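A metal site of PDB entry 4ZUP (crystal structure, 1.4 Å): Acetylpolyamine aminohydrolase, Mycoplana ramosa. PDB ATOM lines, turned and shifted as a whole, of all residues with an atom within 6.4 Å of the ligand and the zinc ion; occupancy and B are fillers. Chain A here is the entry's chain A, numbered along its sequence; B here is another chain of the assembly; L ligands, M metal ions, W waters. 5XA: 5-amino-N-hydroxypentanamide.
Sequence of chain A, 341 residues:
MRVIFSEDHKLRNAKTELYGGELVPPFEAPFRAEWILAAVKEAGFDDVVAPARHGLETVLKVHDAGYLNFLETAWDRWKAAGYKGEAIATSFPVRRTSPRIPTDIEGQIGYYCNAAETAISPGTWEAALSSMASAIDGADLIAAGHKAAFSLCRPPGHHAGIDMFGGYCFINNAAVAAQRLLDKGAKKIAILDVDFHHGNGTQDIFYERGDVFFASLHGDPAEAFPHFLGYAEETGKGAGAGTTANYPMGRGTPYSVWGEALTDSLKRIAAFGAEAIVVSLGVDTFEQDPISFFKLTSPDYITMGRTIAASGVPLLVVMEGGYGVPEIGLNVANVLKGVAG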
ATOM      1  N   GLU A  17      14.756 -16.555  24.491  1.00  0.00           N
ATOM      2  CA  GLU A  17      13.321 -16.524  24.163  1.00  0.00           C
ATOM      3  C   GLU A  17      13.252 -16.371  22.649  1.00  0.00           C
ATOM      4  O   GLU A  17      13.961 -15.527  22.086  1.00  0.00           O
ATOM      5  CB  GLU A  17      12.635 -15.304  24.808  1.00  0.00           C
ATOM      6  CG  GLU A  17      11.212 -15.084  24.332  1.00  0.00           C
ATOM      7  CD  GLU A  17      10.487 -13.960  25.029  1.00  0.00           C
ATOM      8  OE1 GLU A  17      10.909 -13.564  26.137  1.00  0.00           O
ATOM      9  OE2 GLU A  17       9.459 -13.511  24.474  1.00  0.00           O
ATOM     10  N   LEU A  18      12.435 -17.180  22.000  1.00  0.00           N
ATOM     11  CA  LEU A  18      12.218 -17.048  20.569  1.00  0.00           C
ATOM     12  C   LEU A  18      11.209 -15.920  20.330  1.00  0.00           C
ATOM     13  O   LEU A  18      10.035 -16.050  20.684  1.00  0.00           O
ATOM     14  CB  LEU A  18      11.688 -18.375  20.011  1.00  0.00           C
ATOM     15  CG  LEU A  18      11.482 -18.441  18.511  1.00  0.00           C
ATOM     16  CD1 LEU A  18      12.775 -18.126  17.805  1.00  0.00           C
ATOM     17  CD2 LEU A  18      11.013 -19.851  18.179  1.00  0.00           C
ATOM     18  N   TYR A  19      11.678 -14.804  19.769  1.00  0.00           N
ATOM     19  CA  TYR A  19      10.853 -13.628  19.539  1.00  0.00           C
ATOM     20  C   TYR A  19      11.271 -13.014  18.202  1.00  0.00           C
ATOM     21  O   TYR A  19      12.454 -12.734  17.980  1.00  0.00           O
ATOM     22  CB  TYR A  19      11.062 -12.601  20.665  1.00  0.00           C
ATOM     23  CG  TYR A  19      10.324 -11.309  20.422  1.00  0.00           C
ATOM     24  CD1 TYR A  19       8.964 -11.222  20.652  1.00  0.00           C
ATOM     25  CD2 TYR A  19      10.990 -10.167  19.966  1.00  0.00           C
ATOM     26  CE1 TYR A  19       8.267 -10.048  20.429  1.00  0.00           C
ATOM     27  CE2 TYR A  19      10.291  -8.983  19.745  1.00  0.00           C
ATOM     28  CZ  TYR A  19       8.935  -8.940  19.989  1.00  0.00           C
ATOM     29  OH  TYR A  19       8.212  -7.776  19.777  1.00  0.00           O
ATOM     30  N   GLU A 117       7.833 -19.813  22.442  1.00  0.00           N
ATOM     31  CA  GLU A 117       8.530 -18.618  22.913  1.00  0.00           C
ATOM     32  C   GLU A 117       8.911 -18.694  24.396  1.00  0.00           C
ATOM     33  O   GLU A 117       9.298 -17.688  24.995  1.00  0.00           O
ATOM     34  CB  GLU A 117       7.705 -17.355  22.614  1.00  0.00           C
ATOM     35  CG  GLU A 117       6.186 -17.452  22.865  1.00  0.00           C
ATOM     36  CD  GLU A 117       5.826 -17.560  24.347  1.00  0.00           C
ATOM     37  OE1 GLU A 117       5.552 -16.499  24.969  1.00  0.00           O
ATOM     38  OE2 GLU A 117       5.833 -18.677  24.891  1.00  0.00           O
ATOM     39  N   THR A 118       8.798 -19.889  24.982  1.00  0.00           N
ATOM     40  CA  THR A 118       9.226 -20.155  26.353  1.00  0.00           C
ATOM     41  C   THR A 118      10.168 -21.340  26.367  1.00  0.00           C
ATOM     42  O   THR A 118       9.774 -22.477  26.015  1.00  0.00           O
ATOM     43  CB  THR A 118       8.003 -20.470  27.193  1.00  0.00           C
ATOM     44  OG1 THR A 118       7.146 -19.320  27.176  1.00  0.00           O
ATOM     45  CG2 THR A 118       8.378 -20.786  28.633  1.00  0.00           C
ATOM     46  N   PRO A 156       5.473 -16.124  36.191  1.00  0.00           N
ATOM     47  CA  PRO A 156       4.021 -15.987  36.204  1.00  0.00           C
ATOM     48  C   PRO A 156       3.328 -17.305  35.836  1.00  0.00           C
ATOM     49  O   PRO A 156       3.995 -18.316  35.547  1.00  0.00           O
ATOM     50  CB  PRO A 156       3.791 -14.955  35.102  1.00  0.00           C
ATOM     51  CG  PRO A 156       4.928 -15.182  34.144  1.00  0.00           C
ATOM     52  CD  PRO A 156       6.090 -15.474  35.032  1.00  0.00           C
ATOM     53  N   HIS A 158      -0.450 -17.571  34.282  1.00  0.00           N
ATOM     54  CA  HIS A 158      -1.793 -17.692  33.711  1.00  0.00           C
ATOM     55  C   HIS A 158      -1.894 -18.329  32.323  1.00  0.00           C
ATOM     56  O   HIS A 158      -3.004 -18.676  31.900  1.00  0.00           O
ATOM     57  CB  HIS A 158      -2.588 -16.366  33.783  1.00  0.00           C
ATOM     58  CG  HIS A 158      -2.114 -15.293  32.860  1.00  0.00           C
ATOM     59  ND1 HIS A 158      -2.953 -14.296  32.403  1.00  0.00           N
ATOM     60  CD2 HIS A 158      -0.900 -15.031  32.307  1.00  0.00           C
ATOM     61  CE1 HIS A 158      -2.289 -13.480  31.608  1.00  0.00           C
ATOM     62  NE2 HIS A 158      -1.041 -13.898  31.535  1.00  0.00           N
ATOM     63  N   HIS A 159      -0.763 -18.530  31.633  1.00  0.00           N
ATOM     64  CA  HIS A 159      -0.770 -19.265  30.375  1.00  0.00           C
ATOM     65  C   HIS A 159      -0.569 -20.764  30.542  1.00  0.00           C
ATOM     66  O   HIS A 159      -0.679 -21.497  29.568  1.00  0.00           O
ATOM     67  CB  HIS A 159       0.276 -18.700  29.415  1.00  0.00           C
ATOM     68  CG  HIS A 159       0.030 -17.286  29.038  1.00  0.00           C
ATOM     69  ND1 HIS A 159      -1.158 -16.867  28.475  1.00  0.00           N
ATOM     70  CD2 HIS A 159       0.806 -16.189  29.173  1.00  0.00           C
ATOM     71  CE1 HIS A 159      -1.094 -15.562  28.275  1.00  0.00           C
ATOM     72  NE2 HIS A 159       0.093 -15.132  28.672  1.00  0.00           N
ATOM     73  N   GLY A 167       4.013 -19.058  27.203  1.00  0.00           N
ATOM     74  CA  GLY A 167       3.817 -17.668  27.619  1.00  0.00           C
ATOM     75  C   GLY A 167       4.560 -17.291  28.896  1.00  0.00           C
ATOM     76  O   GLY A 167       4.050 -16.505  29.675  1.00  0.00           O
ATOM     77  N   TYR A 168       5.730 -17.900  29.099  1.00  0.00           N
ATOM     78  CA  TYR A 168       6.620 -17.632  30.244  1.00  0.00           C
ATOM     79  C   TYR A 168       6.132 -18.295  31.540  1.00  0.00           C
ATOM     80  O   TYR A 168       6.687 -18.018  32.608  1.00  0.00           O
ATOM     81  CB  TYR A 168       6.778 -16.128  30.488  1.00  0.00           C
ATOM     82  CG  TYR A 168       6.989 -15.230  29.273  1.00  0.00           C
ATOM     83  CD1 TYR A 168       7.502 -15.715  28.058  1.00  0.00           C
ATOM     84  CD2 TYR A 168       6.708 -13.889  29.376  1.00  0.00           C
ATOM     85  CE1 TYR A 168       7.711 -14.851  26.980  1.00  0.00           C
ATOM     86  CE2 TYR A 168       6.907 -13.022  28.320  1.00  0.00           C
ATOM     87  CZ  TYR A 168       7.409 -13.504  27.127  1.00  0.00           C
ATOM     88  OH  TYR A 168       7.634 -12.619  26.081  1.00  0.00           O
ATOM     89  N   CYS A 169       5.107 -19.157  31.422  1.00  0.00           N
ATOM     90  CA  CYS A 169       4.427 -19.743  32.586  1.00  0.00           C
ATOM     91  C   CYS A 169       4.555 -21.265  32.625  1.00  0.00           C
ATOM     92  O   CYS A 169       4.514 -21.932  31.582  1.00  0.00           O
ATOM     93  CB  CYS A 169       2.946 -19.441  32.513  1.00  0.00           C
ATOM     94  SG  CYS A 169       2.532 -17.675  32.435  1.00  0.00           S
ATOM     95  N   ASP A 195      -4.314  -8.862  33.561  1.00  0.00           N
ATOM     96  CA  ASP A 195      -3.154  -8.807  32.680  1.00  0.00           C
ATOM     97  C   ASP A 195      -3.635  -8.549  31.253  1.00  0.00           C
ATOM     98  O   ASP A 195      -4.751  -8.931  30.896  1.00  0.00           O
ATOM     99  CB  ASP A 195      -2.454 -10.159  32.827  1.00  0.00           C
ATOM    100  CG  ASP A 195      -1.176 -10.281  32.022  1.00  0.00           C
ATOM    101  OD1 ASP A 195      -1.237 -10.329  30.763  1.00  0.00           O
ATOM    102  OD2 ASP A 195      -0.082 -10.317  32.658  1.00  0.00           O
ATOM    103  N   PHE A 196      -2.806  -7.879  30.441  1.00  0.00           N
ATOM    104  CA  PHE A 196      -3.178  -7.592  29.057  1.00  0.00           C
ATOM    105  C   PHE A 196      -3.551  -8.860  28.269  1.00  0.00           C
ATOM    106  O   PHE A 196      -4.420  -8.804  27.390  1.00  0.00           O
ATOM    107  CB  PHE A 196      -2.025  -6.896  28.348  1.00  0.00           C
ATOM    108  CG  PHE A 196      -2.218  -6.779  26.862  1.00  0.00           C
ATOM    109  CD1 PHE A 196      -3.120  -5.856  26.340  1.00  0.00           C
ATOM    110  CD2 PHE A 196      -1.541  -7.633  25.995  1.00  0.00           C
ATOM    111  CE1 PHE A 196      -3.297  -5.770  24.949  1.00  0.00           C
ATOM    112  CE2 PHE A 196      -1.703  -7.556  24.621  1.00  0.00           C
ATOM    113  CZ  PHE A 196      -2.600  -6.619  24.091  1.00  0.00           C
ATOM    114  N   HIS A 197      -2.874  -9.966  28.554  1.00  0.00           N
ATOM    115  CA  HIS A 197      -3.090 -11.196  27.785  1.00  0.00           C
ATOM    116  C   HIS A 197      -4.173 -12.053  28.384  1.00  0.00           C
ATOM    117  O   HIS A 197      -4.363 -12.081  29.606  1.00  0.00           O
ATOM    118  CB  HIS A 197      -1.795 -11.996  27.726  1.00  0.00           C
ATOM    119  CG  HIS A 197      -0.662 -11.222  27.141  1.00  0.00           C
ATOM    120  ND1 HIS A 197       0.218 -10.487  27.906  1.00  0.00           N
ATOM    121  CD2 HIS A 197      -0.303 -11.018  25.845  1.00  0.00           C
ATOM    122  CE1 HIS A 197       1.094  -9.889  27.110  1.00  0.00           C
ATOM    123  NE2 HIS A 197       0.807 -10.205  25.857  1.00  0.00           N
ATOM    124  N   HIS A 198      -4.887 -12.761  27.535  1.00  0.00           N
ATOM    125  CA  HIS A 198      -5.867 -13.723  28.017  1.00  0.00           C
ATOM    126  C   HIS A 198      -5.197 -14.782  28.878  1.00  0.00           C
ATOM    127  O   HIS A 198      -4.153 -15.331  28.494  1.00  0.00           O
ATOM    128  CB  HIS A 198      -6.563 -14.413  26.845  1.00  0.00           C
ATOM    129  CG  HIS A 198      -7.618 -15.379  27.273  1.00  0.00           C
ATOM    130  ND1 HIS A 198      -7.581 -16.720  26.951  1.00  0.00           N
ATOM    131  CD2 HIS A 198      -8.734 -15.182  28.012  1.00  0.00           C
ATOM    132  CE1 HIS A 198      -8.656 -17.303  27.465  1.00  0.00           C
ATOM    133  NE2 HIS A 198      -9.360 -16.403  28.138  1.00  0.00           N
ATOM    134  N   PHE A 225      -1.458 -12.327  21.446  1.00  0.00           N
ATOM    135  CA  PHE A 225      -1.129 -13.552  22.186  1.00  0.00           C
ATOM    136  C   PHE A 225      -2.122 -13.685  23.343  1.00  0.00           C
ATOM    137  O   PHE A 225      -2.429 -12.706  24.008  1.00  0.00           O
ATOM    138  CB  PHE A 225       0.314 -13.416  22.740  1.00  0.00           C
ATOM    139  CG  PHE A 225       0.806 -14.664  23.430  1.00  0.00           C
ATOM    140  CD1 PHE A 225       1.523 -15.608  22.729  1.00  0.00           C
ATOM    141  CD2 PHE A 225       0.526 -14.903  24.774  1.00  0.00           C
ATOM    142  CE1 PHE A 225       1.961 -16.767  23.355  1.00  0.00           C
ATOM    143  CE2 PHE A 225       0.944 -16.067  25.392  1.00  0.00           C
ATOM    144  CZ  PHE A 225       1.666 -16.997  24.682  1.00  0.00           C
ATOM    145  N   GLY A 282      -1.443  -8.457  35.844  1.00  0.00           N
ATOM    146  CA  GLY A 282      -0.341  -8.034  35.011  1.00  0.00           C
ATOM    147  C   GLY A 282      -0.500  -6.548  34.757  1.00  0.00           C
ATOM    148  O   GLY A 282      -1.619  -6.044  34.635  1.00  0.00           O
ATOM    149  N   ASP A 284       1.031  -5.177  32.155  1.00  0.00           N
ATOM    150  CA  ASP A 284       1.294  -5.024  30.720  1.00  0.00           C
ATOM    151  C   ASP A 284       0.179  -4.322  29.956  1.00  0.00           C
ATOM    152  O   ASP A 284       0.332  -4.087  28.765  1.00  0.00           O
ATOM    153  CB  ASP A 284       1.708  -6.349  30.037  1.00  0.00           C
ATOM    154  CG  ASP A 284       0.914  -7.554  30.487  1.00  0.00           C
ATOM    155  OD1 ASP A 284      -0.120  -7.393  31.161  1.00  0.00           O
ATOM    156  OD2 ASP A 284       1.366  -8.667  30.073  1.00  0.00           O
ATOM    157  N   ILE A 291       5.163  -5.033  24.697  1.00  0.00           N
ATOM    158  CA  ILE A 291       4.600  -6.116  23.893  1.00  0.00           C
ATOM    159  C   ILE A 291       3.055  -6.061  23.833  1.00  0.00           C
ATOM    160  O   ILE A 291       2.430  -6.979  23.322  1.00  0.00           O
ATOM    161  CB  ILE A 291       5.147  -7.529  24.351  1.00  0.00           C
ATOM    162  CG1 ILE A 291       4.716  -7.875  25.777  1.00  0.00           C
ATOM    163  CG2 ILE A 291       6.698  -7.612  24.153  1.00  0.00           C
ATOM    164  CD1 ILE A 291       4.968  -9.363  26.164  1.00  0.00           C
ATOM    165  N   SER A 292       2.479  -4.950  24.269  1.00  0.00           N
ATOM    166  CA  SER A 292       1.024  -4.869  24.477  1.00  0.00           C
ATOM    167  C   SER A 292       0.418  -3.581  23.896  1.00  0.00           C
ATOM    168  O   SER A 292       1.137  -2.626  23.632  1.00  0.00           O
ATOM    169  CB  SER A 292       0.715  -5.003  25.961  1.00  0.00           C
ATOM    170  OG  SER A 292       1.389  -6.154  26.504  1.00  0.00           O
ATOM    171  N   GLU A 320       1.403 -11.419  37.621  1.00  0.00           N
ATOM    172  CA  GLU A 320       1.544 -12.015  36.276  1.00  0.00           C
ATOM    173  C   GLU A 320       2.570 -11.207  35.473  1.00  0.00           C
ATOM    174  O   GLU A 320       3.722 -11.110  35.878  1.00  0.00           O
ATOM    175  CB  GLU A 320       0.188 -12.119  35.576  1.00  0.00           C
ATOM    176  CG  GLU A 320      -0.882 -12.920  36.374  1.00  0.00           C
ATOM    177  CD  GLU A 320      -0.732 -14.435  36.290  1.00  0.00           C
ATOM    178  OE1 GLU A 320       0.170 -14.957  35.598  1.00  0.00           O
ATOM    179  OE2 GLU A 320      -1.548 -15.136  36.934  1.00  0.00           O
ATOM    180  N   GLY A 321       2.148 -10.609  34.351  1.00  0.00           N
ATOM    181  CA  GLY A 321       3.067  -9.943  33.428  1.00  0.00           C
ATOM    182  C   GLY A 321       3.230  -8.430  33.632  1.00  0.00           C
ATOM    183  O   GLY A 321       2.795  -7.862  34.638  1.00  0.00           O
ATOM    184  N   GLY A 322       3.871  -7.793  32.652  1.00  0.00           N
ATOM    185  CA  GLY A 322       4.264  -6.379  32.758  1.00  0.00           C
ATOM    186  C   GLY A 322       5.752  -6.279  32.551  1.00  0.00           C
ATOM    187  O   GLY A 322       6.525  -6.842  33.339  1.00  0.00           O
ATOM    188  N   TYR A 323       6.185  -5.570  31.501  1.00  0.00           N
ATOM    189  CA  TYR A 323       7.548  -5.676  31.014  1.00  0.00           C
ATOM    190  C   TYR A 323       8.244  -4.369  30.770  1.00  0.00           C
ATOM    191  O   TYR A 323       7.605  -3.313  30.667  1.00  0.00           O
ATOM    192  CB  TYR A 323       7.541  -6.512  29.721  1.00  0.00           C
ATOM    193  CG  TYR A 323       6.870  -7.826  29.991  1.00  0.00           C
ATOM    194  CD1 TYR A 323       7.556  -8.836  30.664  1.00  0.00           C
ATOM    195  CD2 TYR A 323       5.534  -8.020  29.672  1.00  0.00           C
ATOM    196  CE1 TYR A 323       6.927 -10.016  30.979  1.00  0.00           C
ATOM    197  CE2 TYR A 323       4.897  -9.205  29.998  1.00  0.00           C
ATOM    198  CZ  TYR A 323       5.594 -10.194  30.632  1.00  0.00           C
ATOM    199  OH  TYR A 323       4.964 -11.367  30.968  1.00  0.00           O
ATOM    200  N   THR B  90       5.357 -19.176  16.976  1.00  0.00           N
ATOM    201  CA  THR B  90       5.604 -19.496  18.377  1.00  0.00           C
ATOM    202  C   THR B  90       4.358 -20.078  19.051  1.00  0.00           C
ATOM    203  O   THR B  90       4.442 -21.051  19.780  1.00  0.00           O
ATOM    204  CB  THR B  90       6.159 -18.270  19.142  1.00  0.00           C
ATOM    205  OG1 THR B  90       5.326 -17.129  18.908  1.00  0.00           O
ATOM    206  CG2 THR B  90       7.576 -17.936  18.680  1.00  0.00           C
HETATM  207  O8  5XA L   1       0.651 -12.375  30.339  1.00  0.00           O
HETATM  208  N7  5XA L   1       1.515 -13.002  29.444  1.00  0.00           N
HETATM  209  C6  5XA L   1       2.550 -12.273  29.117  1.00  0.00           C
HETATM  210  O9  5XA L   1       2.702 -11.152  29.593  1.00  0.00           O
HETATM  211  C5  5XA L   1       3.518 -12.934  28.187  1.00  0.00           C
HETATM  212  C4  5XA L   1       3.122 -12.899  26.730  1.00  0.00           C
HETATM  213  C3  5XA L   1       4.112 -13.812  25.996  1.00  0.00           C
HETATM  214  C2  5XA L   1       4.012 -13.629  24.499  1.00  0.00           C
HETATM  215  N1  5XA L   1       5.178 -14.260  23.898  1.00  0.00           N
HETATM  216 ZN    ZN M   1       0.576 -10.436  29.967  1.00  0.00          ZN
HETATM  217  O   HOH W   1       2.578 -13.966  31.933  1.00  0.00           O
HETATM  218  O   HOH W   2       6.592 -11.409  23.564  1.00  0.00           O
HETATM  219  O   HOH W   3       4.242 -13.339  21.340  1.00  0.00           O
HETATM  220  O   HOH W   4       7.983 -14.056  22.274  1.00  0.00           O
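Water W1 bridges a nitrogen (N7) of the ligand (2.9 Å) and the side-chain sulfur of Cys 169 (3.7 Å).
Water W2 lies within hydrogen-bond range of OH of Tyr 168 (3.0 Å) and N1 of the ligand (3.2 Å).
Water W4 lies within hydrogen-bond range of OE2 of Glu 17, N1 of the ligand and O of Leu 18.
OD2 of Asp 284 is bound to the zinc ion, 1.9 Å away.
The zinc ion is bound by O8 of the ligand.
OD1 of Asp 195 is bound to the zinc ion, at 2.0 Å.
The zinc ion is bound by ND1 of His 197 (2.1 Å).
An oxygen (O9) of the ligand binds the zinc ion, 2.3 Å away.
The zinc ion has five donor atoms within binding distance.
Slightly farther from the zinc ion lies the side-chain carboxylate (OD2) of Asp 195 (2.8 Å).
Within 4 Å of the zinc ion: Asp 195, His 197 and Asp 284.
The nearest printed residue that does not touch the zinc ion is His 158 (4.1 Å).
The side-chain carboxylate (OE1) of Glu 117 is in salt-bridge range of a nitrogen (N1) of the ligand, 2.5 Å away.
A nitrogen (N7) of the ligand is in hydrogen-bond range of a ring nitrogen (NE2) of His 158, 3.4 Å away.
O9 of the ligand sits close to OH of Tyr 323 (2.7 Å).
A nitrogen (N7) of the ligand lies within hydrogen-bond range of a ring nitrogen (NE2) of His 159 (2.7 Å).
Merely in contact with the ligand: Gly 167 (3.9 Å), Tyr 168 (3.4 Å) and Phe 225 (3.5 Å).
Hydrophobic or aromatic side chains that line the ligand: His 158, His 159, Tyr 168, His 197, Phe 225 and Tyr 323.
Within 4 Å of the ligand: Glu 117, His 158, His 159, Gly 167, Tyr 168, Asp 195, His 197, Phe 225, Asp 284 and Tyr 323.
The side-chain carboxylate (OD1) of Asp 284 lies within hydrogen-bond range of the backbone NH (N) of Phe 196, 2.8 Å away.
The side-chain hydroxyl of Ser 292 sits close to the backbone carbonyl oxygen of Asp 284 (3.2 Å).
OE2 of Glu 117 is in hydrogen-bond range of OG1 of Thr 118 (2.7 Å).
The side-chain carboxylate of Glu 320 is in hydrogen-bond range of the backbone NH of His 158 (3.0 Å).
ND1 of His 159 lies close to O of His 198, at 3.4 Å.
OE2 of Glu 17 is in hydrogen-bond range of OH of Tyr 168 (2.6 Å).
The backbone NH (N) of Tyr 168 is in hydrogen-bond range of the side-chain hydroxyl (OG1) of Thr 118 (2.8 Å).
SG of Cys 169 lies within hydrogen-bond range of O of Gly 167.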
